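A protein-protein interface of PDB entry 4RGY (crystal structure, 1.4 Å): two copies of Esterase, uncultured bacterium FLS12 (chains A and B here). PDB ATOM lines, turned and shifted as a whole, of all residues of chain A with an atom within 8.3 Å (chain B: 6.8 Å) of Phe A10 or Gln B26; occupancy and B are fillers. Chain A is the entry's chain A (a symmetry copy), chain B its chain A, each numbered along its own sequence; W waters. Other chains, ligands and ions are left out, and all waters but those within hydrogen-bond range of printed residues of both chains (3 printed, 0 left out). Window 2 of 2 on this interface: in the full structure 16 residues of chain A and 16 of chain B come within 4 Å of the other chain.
The backbone NH of Asp A8 sits at hydrogen-bond distance from the backbone carbonyl oxygen of Leu B4 (2.8 Å). The side-chain amide nitrogen (NE2) of Gln B26 sits close to the backbone NH (N) of Phe A10 (2.8 Å).
O of Leu A106 sits at hydrogen-bond distance from OG of Ser A109, at 2.8 Å. The backbone carbonyl oxygen (O) of Phe A9 sits at hydrogen-bond distance from the backbone NH (N) of Thr A18, 2.9 Å away. O of His B1 sits at hydrogen-bond distance from N of Gln B26 (3.0 Å). The side-chain carboxylate of Asp A8 is in hydrogen-bond range of the side-chain hydroxyl of Ser A19, at 2.6 Å. The backbone NH of Ala B3 sits at hydrogen-bond distance from the backbone carbonyl oxygen of Leu B24 (2.8 Å).
Cys A7 touches Leu B4. O of Asp A8 touches CA of Ala B3, 3.6 Å away. Phe A9 touches Gln B26. His B1 touches Phe A10 (NE2 to CD2, 3.3 Å). Gln B26 touches Leu A106. Ser A109 touches Glu B27 (CB to OE2, 3.5 Å). Phe A110 touches Ala B3 (CZ to CB, 3.8 Å).
Phe A10 touches two residues of chain B. Leu A16 touches none of the printed residues of chain B. Of the printed residues of chain B, Leu A106 touches Gln B26 (3.98 Å). Printed residues of chain A within 4 Å of His B1: Phe A10 (3.3 Å). Of the printed residues of chain A, Gln B26 touches Phe A9 (3.5 Å), Phe A10 (2.8 Å) and Leu A106 (3.98 Å). Of the printed residues of chain A, Glu B27 touches Ser A109. The nearest residue of chain B that does not touch Phe A10 is Met B2 (5.3 Å). The nearest printed residue of chain B that does not touch Ser A109 is Leu B24 (5.2 Å).
Printed residues of chain A that touch a printed residue of chain B: Cys A7, Asp A8, Phe A9, Phe A10, Leu A106, Ser A109 and Phe A110. Hydrophobic or aromatic side chains of chain A that line the printed part of chain B: Phe A9, Phe A10, Leu A106 and Phe A110.
No position is printed for both chains.
Water W3 lies within hydrogen-bond range of the backbone carbonyl oxygen (O) of Met B2 (2.5 Å), the side-chain amide nitrogen (NE2) of Gln B26 (3.1 Å) and the backbone NH (N) of Phe A10 (3.2 Å). Water W2 bridges the backbone NH (N) of Glu B27 (2.8 Å) and the side-chain hydroxyl (OG) of Ser A109 (2.9 Å). Water W1 lies within hydrogen-bond range of the side-chain carboxylate of Glu B27 (2.9 Å) and the backbone carbonyl oxygen of Ser A109 (3.0 Å).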
ATOM      1  N   CYS A   7      20.114  -8.472  31.122  1.00  0.00           N
ATOM      2  CA  CYS A   7      21.129  -8.423  30.081  1.00  0.00           C
ATOM      3  C   CYS A   7      21.049  -9.655  29.214  1.00  0.00           C
ATOM      4  O   CYS A   7      21.227 -10.777  29.707  1.00  0.00           O
ATOM      5  CB  CYS A   7      22.523  -8.388  30.723  1.00  0.00           C
ATOM      6  SG  CYS A   7      22.710  -7.257  32.134  1.00  0.00           S
ATOM      7  N   ASP A   8      20.807  -9.460  27.923  1.00  0.00           N
ATOM      8  CA  ASP A   8      20.795 -10.549  26.962  1.00  0.00           C
ATOM      9  C   ASP A   8      22.014 -10.395  26.062  1.00  0.00           C
ATOM     10  O   ASP A   8      22.085  -9.471  25.246  1.00  0.00           O
ATOM     11  CB  ASP A   8      19.506 -10.531  26.149  1.00  0.00           C
ATOM     12  CG  ASP A   8      18.285 -10.664  27.016  1.00  0.00           C
ATOM     13  OD1 ASP A   8      18.309 -11.512  27.924  1.00  0.00           O
ATOM     14  OD2 ASP A   8      17.313  -9.906  26.809  1.00  0.00           O
ATOM     15  N   PHE A   9      22.968 -11.313  26.207  1.00  0.00           N
ATOM     16  CA  PHE A   9      24.281 -11.166  25.596  1.00  0.00           C
ATOM     17  C   PHE A   9      24.730 -12.500  25.021  1.00  0.00           C
ATOM     18  O   PHE A   9      24.106 -13.532  25.257  1.00  0.00           O
ATOM     19  CB  PHE A   9      25.300 -10.691  26.644  1.00  0.00           C
ATOM     20  CG  PHE A   9      25.518 -11.678  27.757  1.00  0.00           C
ATOM     21  CD1 PHE A   9      24.680 -11.695  28.865  1.00  0.00           C
ATOM     22  CD2 PHE A   9      26.553 -12.599  27.693  1.00  0.00           C
ATOM     23  CE1 PHE A   9      24.871 -12.623  29.884  1.00  0.00           C
ATOM     24  CE2 PHE A   9      26.751 -13.528  28.708  1.00  0.00           C
ATOM     25  CZ  PHE A   9      25.904 -13.535  29.802  1.00  0.00           C
ATOM     26  N   PHE A  10      25.823 -12.480  24.269  1.00  0.00           N
ATOM     27  CA  PHE A  10      26.330 -13.700  23.664  1.00  0.00           C
ATOM     28  C   PHE A  10      27.544 -14.229  24.398  1.00  0.00           C
ATOM     29  O   PHE A  10      28.491 -13.480  24.669  1.00  0.00           O
ATOM     30  CB  PHE A  10      26.685 -13.474  22.184  1.00  0.00           C
ATOM     31  CG  PHE A  10      26.995 -14.748  21.448  1.00  0.00           C
ATOM     32  CD1 PHE A  10      25.965 -15.549  20.986  1.00  0.00           C
ATOM     33  CD2 PHE A  10      28.306 -15.149  21.234  1.00  0.00           C
ATOM     34  CE1 PHE A  10      26.228 -16.730  20.320  1.00  0.00           C
ATOM     35  CE2 PHE A  10      28.583 -16.331  20.563  1.00  0.00           C
ATOM     36  CZ  PHE A  10      27.536 -17.117  20.099  1.00  0.00           C
ATOM     37  N   SER A  11      27.522 -15.523  24.711  1.00  0.00           N
ATOM     38  CA  SER A  11      28.689 -16.178  25.281  1.00  0.00           C
ATOM     39  C   SER A  11      29.453 -16.930  24.198  1.00  0.00           C
ATOM     40  O   SER A  11      28.945 -17.891  23.610  1.00  0.00           O
ATOM     41  CB  SER A  11      28.301 -17.150  26.396  1.00  0.00           C
ATOM     42  OG  SER A  11      29.417 -17.966  26.720  1.00  0.00           O
ATOM     43  N   ASP A  12      30.676 -16.480  23.935  1.00  0.00           N
ATOM     44  CA  ASP A  12      31.571 -17.158  23.010  1.00  0.00           C
ATOM     45  C   ASP A  12      32.002 -18.529  23.536  1.00  0.00           C
ATOM     46  O   ASP A  12      32.123 -19.486  22.776  1.00  0.00           O
ATOM     47  CB  ASP A  12      32.797 -16.281  22.742  1.00  0.00           C
ATOM     48  CG  ASP A  12      32.499 -15.151  21.774  1.00  0.00           C
ATOM     49  OD1 ASP A  12      32.087 -15.451  20.632  1.00  0.00           O
ATOM     50  OD2 ASP A  12      32.660 -13.970  22.154  1.00  0.00           O
ATOM     51  N   VAL A  13      32.208 -18.625  24.847  1.00  0.00           N
ATOM     52  CA  VAL A  13      32.606 -19.896  25.441  1.00  0.00           C
ATOM     53  C   VAL A  13      31.514 -20.949  25.298  1.00  0.00           C
ATOM     54  O   VAL A  13      31.804 -22.104  24.983  1.00  0.00           O
ATOM     55  CB  VAL A  13      32.987 -19.714  26.921  1.00  0.00           C
ATOM     56  CG1 VAL A  13      33.059 -21.061  27.644  1.00  0.00           C
ATOM     57  CG2 VAL A  13      34.315 -18.961  27.027  1.00  0.00           C
ATOM     58  N   LEU A  14      30.264 -20.551  25.529  1.00  0.00           N
ATOM     59  CA  LEU A  14      29.140 -21.479  25.430  1.00  0.00           C
ATOM     60  C   LEU A  14      28.646 -21.614  23.995  1.00  0.00           C
ATOM     61  O   LEU A  14      27.963 -22.581  23.655  1.00  0.00           O
ATOM     62  CB  LEU A  14      27.986 -21.031  26.324  1.00  0.00           C
ATOM     63  CG  LEU A  14      28.259 -20.916  27.823  1.00  0.00           C
ATOM     64  CD1 LEU A  14      27.033 -20.384  28.564  1.00  0.00           C
ATOM     65  CD2 LEU A  14      28.662 -22.274  28.371  1.00  0.00           C
ATOM     66  N   GLY A  15      28.977 -20.635  23.158  1.00  0.00           N
ATOM     67  CA  GLY A  15      28.423 -20.577  21.813  1.00  0.00           C
ATOM     68  C   GLY A  15      26.917 -20.372  21.909  1.00  0.00           C
ATOM     69  O   GLY A  15      26.142 -21.028  21.200  1.00  0.00           O
ATOM     70  N   LEU A  16      26.490 -19.464  22.784  1.00  0.00           N
ATOM     71  CA  LEU A  16      25.068 -19.361  23.100  1.00  0.00           C
ATOM     72  C   LEU A  16      24.669 -17.980  23.577  1.00  0.00           C
ATOM     73  O   LEU A  16      25.339 -17.386  24.440  1.00  0.00           O
ATOM     74  CB  LEU A  16      24.698 -20.401  24.162  1.00  0.00           C
ATOM     75  CG  LEU A  16      23.233 -20.524  24.590  1.00  0.00           C
ATOM     76  CD1 LEU A  16      22.367 -20.965  23.429  1.00  0.00           C
ATOM     77  CD2 LEU A  16      23.120 -21.525  25.735  1.00  0.00           C
ATOM     78  N   SER A  17      23.554 -17.494  23.042  1.00  0.00           N
ATOM     79  CA  SER A  17      22.896 -16.291  23.537  1.00  0.00           C
ATOM     80  C   SER A  17      22.243 -16.636  24.862  1.00  0.00           C
ATOM     81  O   SER A  17      21.499 -17.623  24.964  1.00  0.00           O
ATOM     82  CB  SER A  17      21.817 -15.837  22.560  1.00  0.00           C
ATOM     83  OG  SER A  17      22.385 -15.351  21.358  1.00  0.00           O
ATOM     84  N   THR A  18      22.526 -15.843  25.886  1.00  0.00           N
ATOM     85  CA  THR A  18      22.035 -16.156  27.216  1.00  0.00           C
ATOM     86  C   THR A  18      21.765 -14.853  27.967  1.00  0.00           C
ATOM     87  O   THR A  18      21.771 -13.774  27.369  1.00  0.00           O
ATOM     88  CB  THR A  18      23.028 -17.118  27.924  1.00  0.00           C
ATOM     89  OG1 THR A  18      22.482 -17.561  29.175  1.00  0.00           O
ATOM     90  CG2 THR A  18      24.366 -16.427  28.136  1.00  0.00           C
ATOM     91  N   SER A  19      21.485 -14.953  29.262  1.00  0.00           N
ATOM     92  CA  SER A  19      21.047 -13.796  30.022  1.00  0.00           C
ATOM     93  C   SER A  19      21.657 -13.761  31.408  1.00  0.00           C
ATOM     94  O   SER A  19      22.026 -14.800  31.947  1.00  0.00           O
ATOM     95  CB  SER A  19      19.526 -13.818  30.170  1.00  0.00           C
ATOM     96  OG  SER A  19      18.913 -13.811  28.899  1.00  0.00           O
ATOM     97  N   PHE A  98      33.080 -20.687  31.355  1.00  0.00           N
ATOM     98  CA  PHE A  98      32.163 -19.561  31.309  1.00  0.00           C
ATOM     99  C   PHE A  98      32.120 -18.827  32.652  1.00  0.00           C
ATOM    100  O   PHE A  98      32.350 -17.612  32.719  1.00  0.00           O
ATOM    101  CB  PHE A  98      30.761 -20.052  30.923  1.00  0.00           C
ATOM    102  CG  PHE A  98      29.694 -18.996  31.038  1.00  0.00           C
ATOM    103  CD1 PHE A  98      29.686 -17.892  30.182  1.00  0.00           C
ATOM    104  CD2 PHE A  98      28.691 -19.111  31.995  1.00  0.00           C
ATOM    105  CE1 PHE A  98      28.702 -16.922  30.281  1.00  0.00           C
ATOM    106  CE2 PHE A  98      27.698 -18.144  32.095  1.00  0.00           C
ATOM    107  CZ  PHE A  98      27.704 -17.048  31.236  1.00  0.00           C
ATOM    108  N   GLU A 102      34.919 -16.121  31.312  1.00  0.00           N
ATOM    109  CA  GLU A 102      34.204 -15.234  30.403  1.00  0.00           C
ATOM    110  C   GLU A 102      33.177 -14.341  31.082  1.00  0.00           C
ATOM    111  O   GLU A 102      33.080 -13.147  30.790  1.00  0.00           O
ATOM    112  CB  GLU A 102      33.529 -16.017  29.284  1.00  0.00           C
ATOM    113  CG  GLU A 102      33.072 -15.103  28.157  1.00  0.00           C
ATOM    114  CD  GLU A 102      32.229 -15.804  27.125  1.00  0.00           C
ATOM    115  OE1 GLU A 102      31.505 -16.751  27.482  1.00  0.00           O
ATOM    116  OE2 GLU A 102      32.280 -15.390  25.949  1.00  0.00           O
ATOM    117  N   LEU A 106      32.924 -10.354  30.926  1.00  0.00           N
ATOM    118  CA  LEU A 106      31.816  -9.686  30.250  1.00  0.00           C
ATOM    119  C   LEU A 106      31.128  -8.687  31.173  1.00  0.00           C
ATOM    120  O   LEU A 106      30.820  -7.560  30.781  1.00  0.00           O
ATOM    121  CB  LEU A 106      30.804 -10.709  29.732  1.00  0.00           C
ATOM    122  CG  LEU A 106      31.243 -11.519  28.508  1.00  0.00           C
ATOM    123  CD1 LEU A 106      30.282 -12.664  28.253  1.00  0.00           C
ATOM    124  CD2 LEU A 106      31.363 -10.643  27.263  1.00  0.00           C
ATOM    125  N   SER A 109      33.210  -5.682  31.463  1.00  0.00           N
ATOM    126  CA  SER A 109      33.247  -4.918  30.218  1.00  0.00           C
ATOM    127  C   SER A 109      31.985  -4.059  30.056  1.00  0.00           C
ATOM    128  O   SER A 109      32.043  -2.955  29.512  1.00  0.00           O
ATOM    129  CB  SER A 109      33.431  -5.847  29.014  1.00  0.00           C
ATOM    130  OG  SER A 109      32.206  -6.440  28.604  1.00  0.00           O
ATOM    131  N   PHE A 110      30.850  -4.550  30.556  1.00  0.00           N
ATOM    132  CA  PHE A 110      29.585  -3.832  30.420  1.00  0.00           C
ATOM    133  C   PHE A 110      29.396  -2.763  31.499  1.00  0.00           C
ATOM    134  O   PHE A 110      28.842  -1.685  31.244  1.00  0.00           O
ATOM    135  CB  PHE A 110      28.401  -4.795  30.555  1.00  0.00           C
ATOM    136  CG  PHE A 110      28.332  -5.870  29.504  1.00  0.00           C
ATOM    137  CD1 PHE A 110      28.908  -5.710  28.252  1.00  0.00           C
ATOM    138  CD2 PHE A 110      27.646  -7.050  29.776  1.00  0.00           C
ATOM    139  CE1 PHE A 110      28.814  -6.722  27.297  1.00  0.00           C
ATOM    140  CE2 PHE A 110      27.552  -8.059  28.837  1.00  0.00           C
ATOM    141  CZ  PHE A 110      28.138  -7.901  27.598  1.00  0.00           C
ATOM    142  N   HIS B   1      28.450  -9.171  17.678  1.00  0.00           N
ATOM    143  CA  HIS B   1      27.390  -9.337  18.668  1.00  0.00           C
ATOM    144  C   HIS B   1      27.106  -8.038  19.398  1.00  0.00           C
ATOM    145  O   HIS B   1      28.024  -7.296  19.756  1.00  0.00           O
ATOM    146  CB  HIS B   1      27.748 -10.440  19.671  1.00  0.00           C
ATOM    147  CG  HIS B   1      27.810 -11.804  19.061  1.00  0.00           C
ATOM    148  ND1 HIS B   1      26.684 -12.489  18.661  1.00  0.00           N
ATOM    149  CD2 HIS B   1      28.862 -12.602  18.772  1.00  0.00           C
ATOM    150  CE1 HIS B   1      27.042 -13.658  18.155  1.00  0.00           C
ATOM    151  NE2 HIS B   1      28.357 -13.750  18.211  1.00  0.00           N
ATOM    152  N   MET B   2      25.823  -7.762  19.602  1.00  0.00           N
ATOM    153  CA  MET B   2      25.406  -6.663  20.450  1.00  0.00           C
ATOM    154  C   MET B   2      24.764  -7.259  21.695  1.00  0.00           C
ATOM    155  O   MET B   2      24.047  -8.264  21.626  1.00  0.00           O
ATOM    156  CB  MET B   2      24.394  -5.762  19.737  1.00  0.00           C
ATOM    157  CG  MET B   2      24.870  -5.169  18.412  1.00  0.00           C
ATOM    158  SD  MET B   2      25.940  -3.736  18.628  1.00  0.00           S
ATOM    159  CE  MET B   2      24.855  -2.604  19.487  1.00  0.00           C
ATOM    160  N   ALA B   3      25.049  -6.657  22.835  1.00  0.00           N
ATOM    161  CA  ALA B   3      24.402  -7.039  24.076  1.00  0.00           C
ATOM    162  C   ALA B   3      23.218  -6.092  24.287  1.00  0.00           C
ATOM    163  O   ALA B   3      23.334  -4.876  24.074  1.00  0.00           O
ATOM    164  CB  ALA B   3      25.377  -6.937  25.214  1.00  0.00           C
ATOM    165  N   LEU B   4      22.087  -6.654  24.718  1.00  0.00           N
ATOM    166  CA  LEU B   4      20.853  -5.907  24.942  1.00  0.00           C
ATOM    167  C   LEU B   4      20.578  -5.751  26.432  1.00  0.00           C
ATOM    168  O   LEU B   4      20.644  -6.722  27.185  1.00  0.00           O
ATOM    169  CB  LEU B   4      19.686  -6.649  24.277  1.00  0.00           C
ATOM    170  CG  LEU B   4      18.278  -6.104  24.529  1.00  0.00           C
ATOM    171  CD1 LEU B   4      18.099  -4.777  23.852  1.00  0.00           C
ATOM    172  CD2 LEU B   4      17.216  -7.083  24.050  1.00  0.00           C
ATOM    173  N   LEU B  24      24.684  -2.394  23.260  1.00  0.00           N
ATOM    174  CA  LEU B  24      26.119  -2.139  23.338  1.00  0.00           C
ATOM    175  C   LEU B  24      26.836  -3.125  22.451  1.00  0.00           C
ATOM    176  O   LEU B  24      26.493  -4.306  22.438  1.00  0.00           O
ATOM    177  CB  LEU B  24      26.633  -2.418  24.750  1.00  0.00           C
ATOM    178  CG  LEU B  24      26.726  -1.423  25.887  1.00  0.00           C
ATOM    179  CD1 LEU B  24      27.556  -2.058  27.013  1.00  0.00           C
ATOM    180  CD2 LEU B  24      27.342  -0.107  25.424  1.00  0.00           C
ATOM    181  N   PRO B  25      27.867  -2.665  21.733  1.00  0.00           N
ATOM    182  CA  PRO B  25      28.731  -3.635  21.065  1.00  0.00           C
ATOM    183  C   PRO B  25      29.460  -4.489  22.098  1.00  0.00           C
ATOM    184  O   PRO B  25      29.857  -3.971  23.141  1.00  0.00           O
ATOM    185  CB  PRO B  25      29.734  -2.748  20.315  1.00  0.00           C
ATOM    186  CG  PRO B  25      29.059  -1.391  20.209  1.00  0.00           C
ATOM    187  CD  PRO B  25      28.261  -1.270  21.464  1.00  0.00           C
ATOM    188  N   GLN B  26      29.611  -5.779  21.814  1.00  0.00           N
ATOM    189  CA  GLN B  26      30.408  -6.660  22.668  1.00  0.00           C
ATOM    190  C   GLN B  26      31.855  -6.703  22.188  1.00  0.00           C
ATOM    191  O   GLN B  26      32.110  -6.741  20.990  1.00  0.00           O
ATOM    192  CB  GLN B  26      29.842  -8.081  22.674  1.00  0.00           C
ATOM    193  CG  GLN B  26      28.646  -8.260  23.576  1.00  0.00           C
ATOM    194  CD  GLN B  26      28.256  -9.717  23.757  1.00  0.00           C
ATOM    195  OE1 GLN B  26      29.098 -10.589  23.988  1.00  0.00           O
ATOM    196  NE2 GLN B  26      26.975  -9.986  23.640  1.00  0.00           N
ATOM    197  N   GLU B  27      32.796  -6.695  23.127  1.00  0.00           N
ATOM    198  CA  GLU B  27      34.215  -6.757  22.781  1.00  0.00           C
ATOM    199  C   GLU B  27      34.588  -8.128  22.232  1.00  0.00           C
ATOM    200  O   GLU B  27      33.888  -9.112  22.479  1.00  0.00           O
ATOM    201  CB  GLU B  27      35.080  -6.427  24.001  1.00  0.00           C
ATOM    202  CG  GLU B  27      34.823  -5.048  24.588  1.00  0.00           C
ATOM    203  CD  GLU B  27      35.910  -4.608  25.550  1.00  0.00           C
ATOM    204  OE1 GLU B  27      37.091  -4.583  25.141  1.00  0.00           O
ATOM    205  OE2 GLU B  27      35.587  -4.291  26.715  1.00  0.00           O
ATOM    206  N   HIS B  43      32.275   3.947  23.707  1.00  0.00           N
ATOM    207  CA  HIS B  43      31.604   3.783  22.430  1.00  0.00           C
ATOM    208  C   HIS B  43      30.873   5.045  22.029  1.00  0.00           C
ATOM    209  O   HIS B  43      30.186   5.639  22.846  1.00  0.00           O
ATOM    210  CB  HIS B  43      30.601   2.631  22.510  1.00  0.00           C
ATOM    211  CG  HIS B  43      31.247   1.281  22.559  1.00  0.00           C
ATOM    212  ND1 HIS B  43      31.864   0.722  21.464  1.00  0.00           N
ATOM    213  CD2 HIS B  43      31.380   0.387  23.567  1.00  0.00           C
ATOM    214  CE1 HIS B  43      32.348  -0.464  21.788  1.00  0.00           C
ATOM    215  NE2 HIS B  43      32.073  -0.692  23.062  1.00  0.00           N
HETATM  216  O   HOH W   1      33.317  -2.485  26.852  1.00  0.00           O
HETATM  217  O   HOH W   2      31.997  -6.931  25.758  1.00  0.00           O
HETATM  218  O   HOH W   3      24.332 -10.643  22.139  1.00  0.00           O
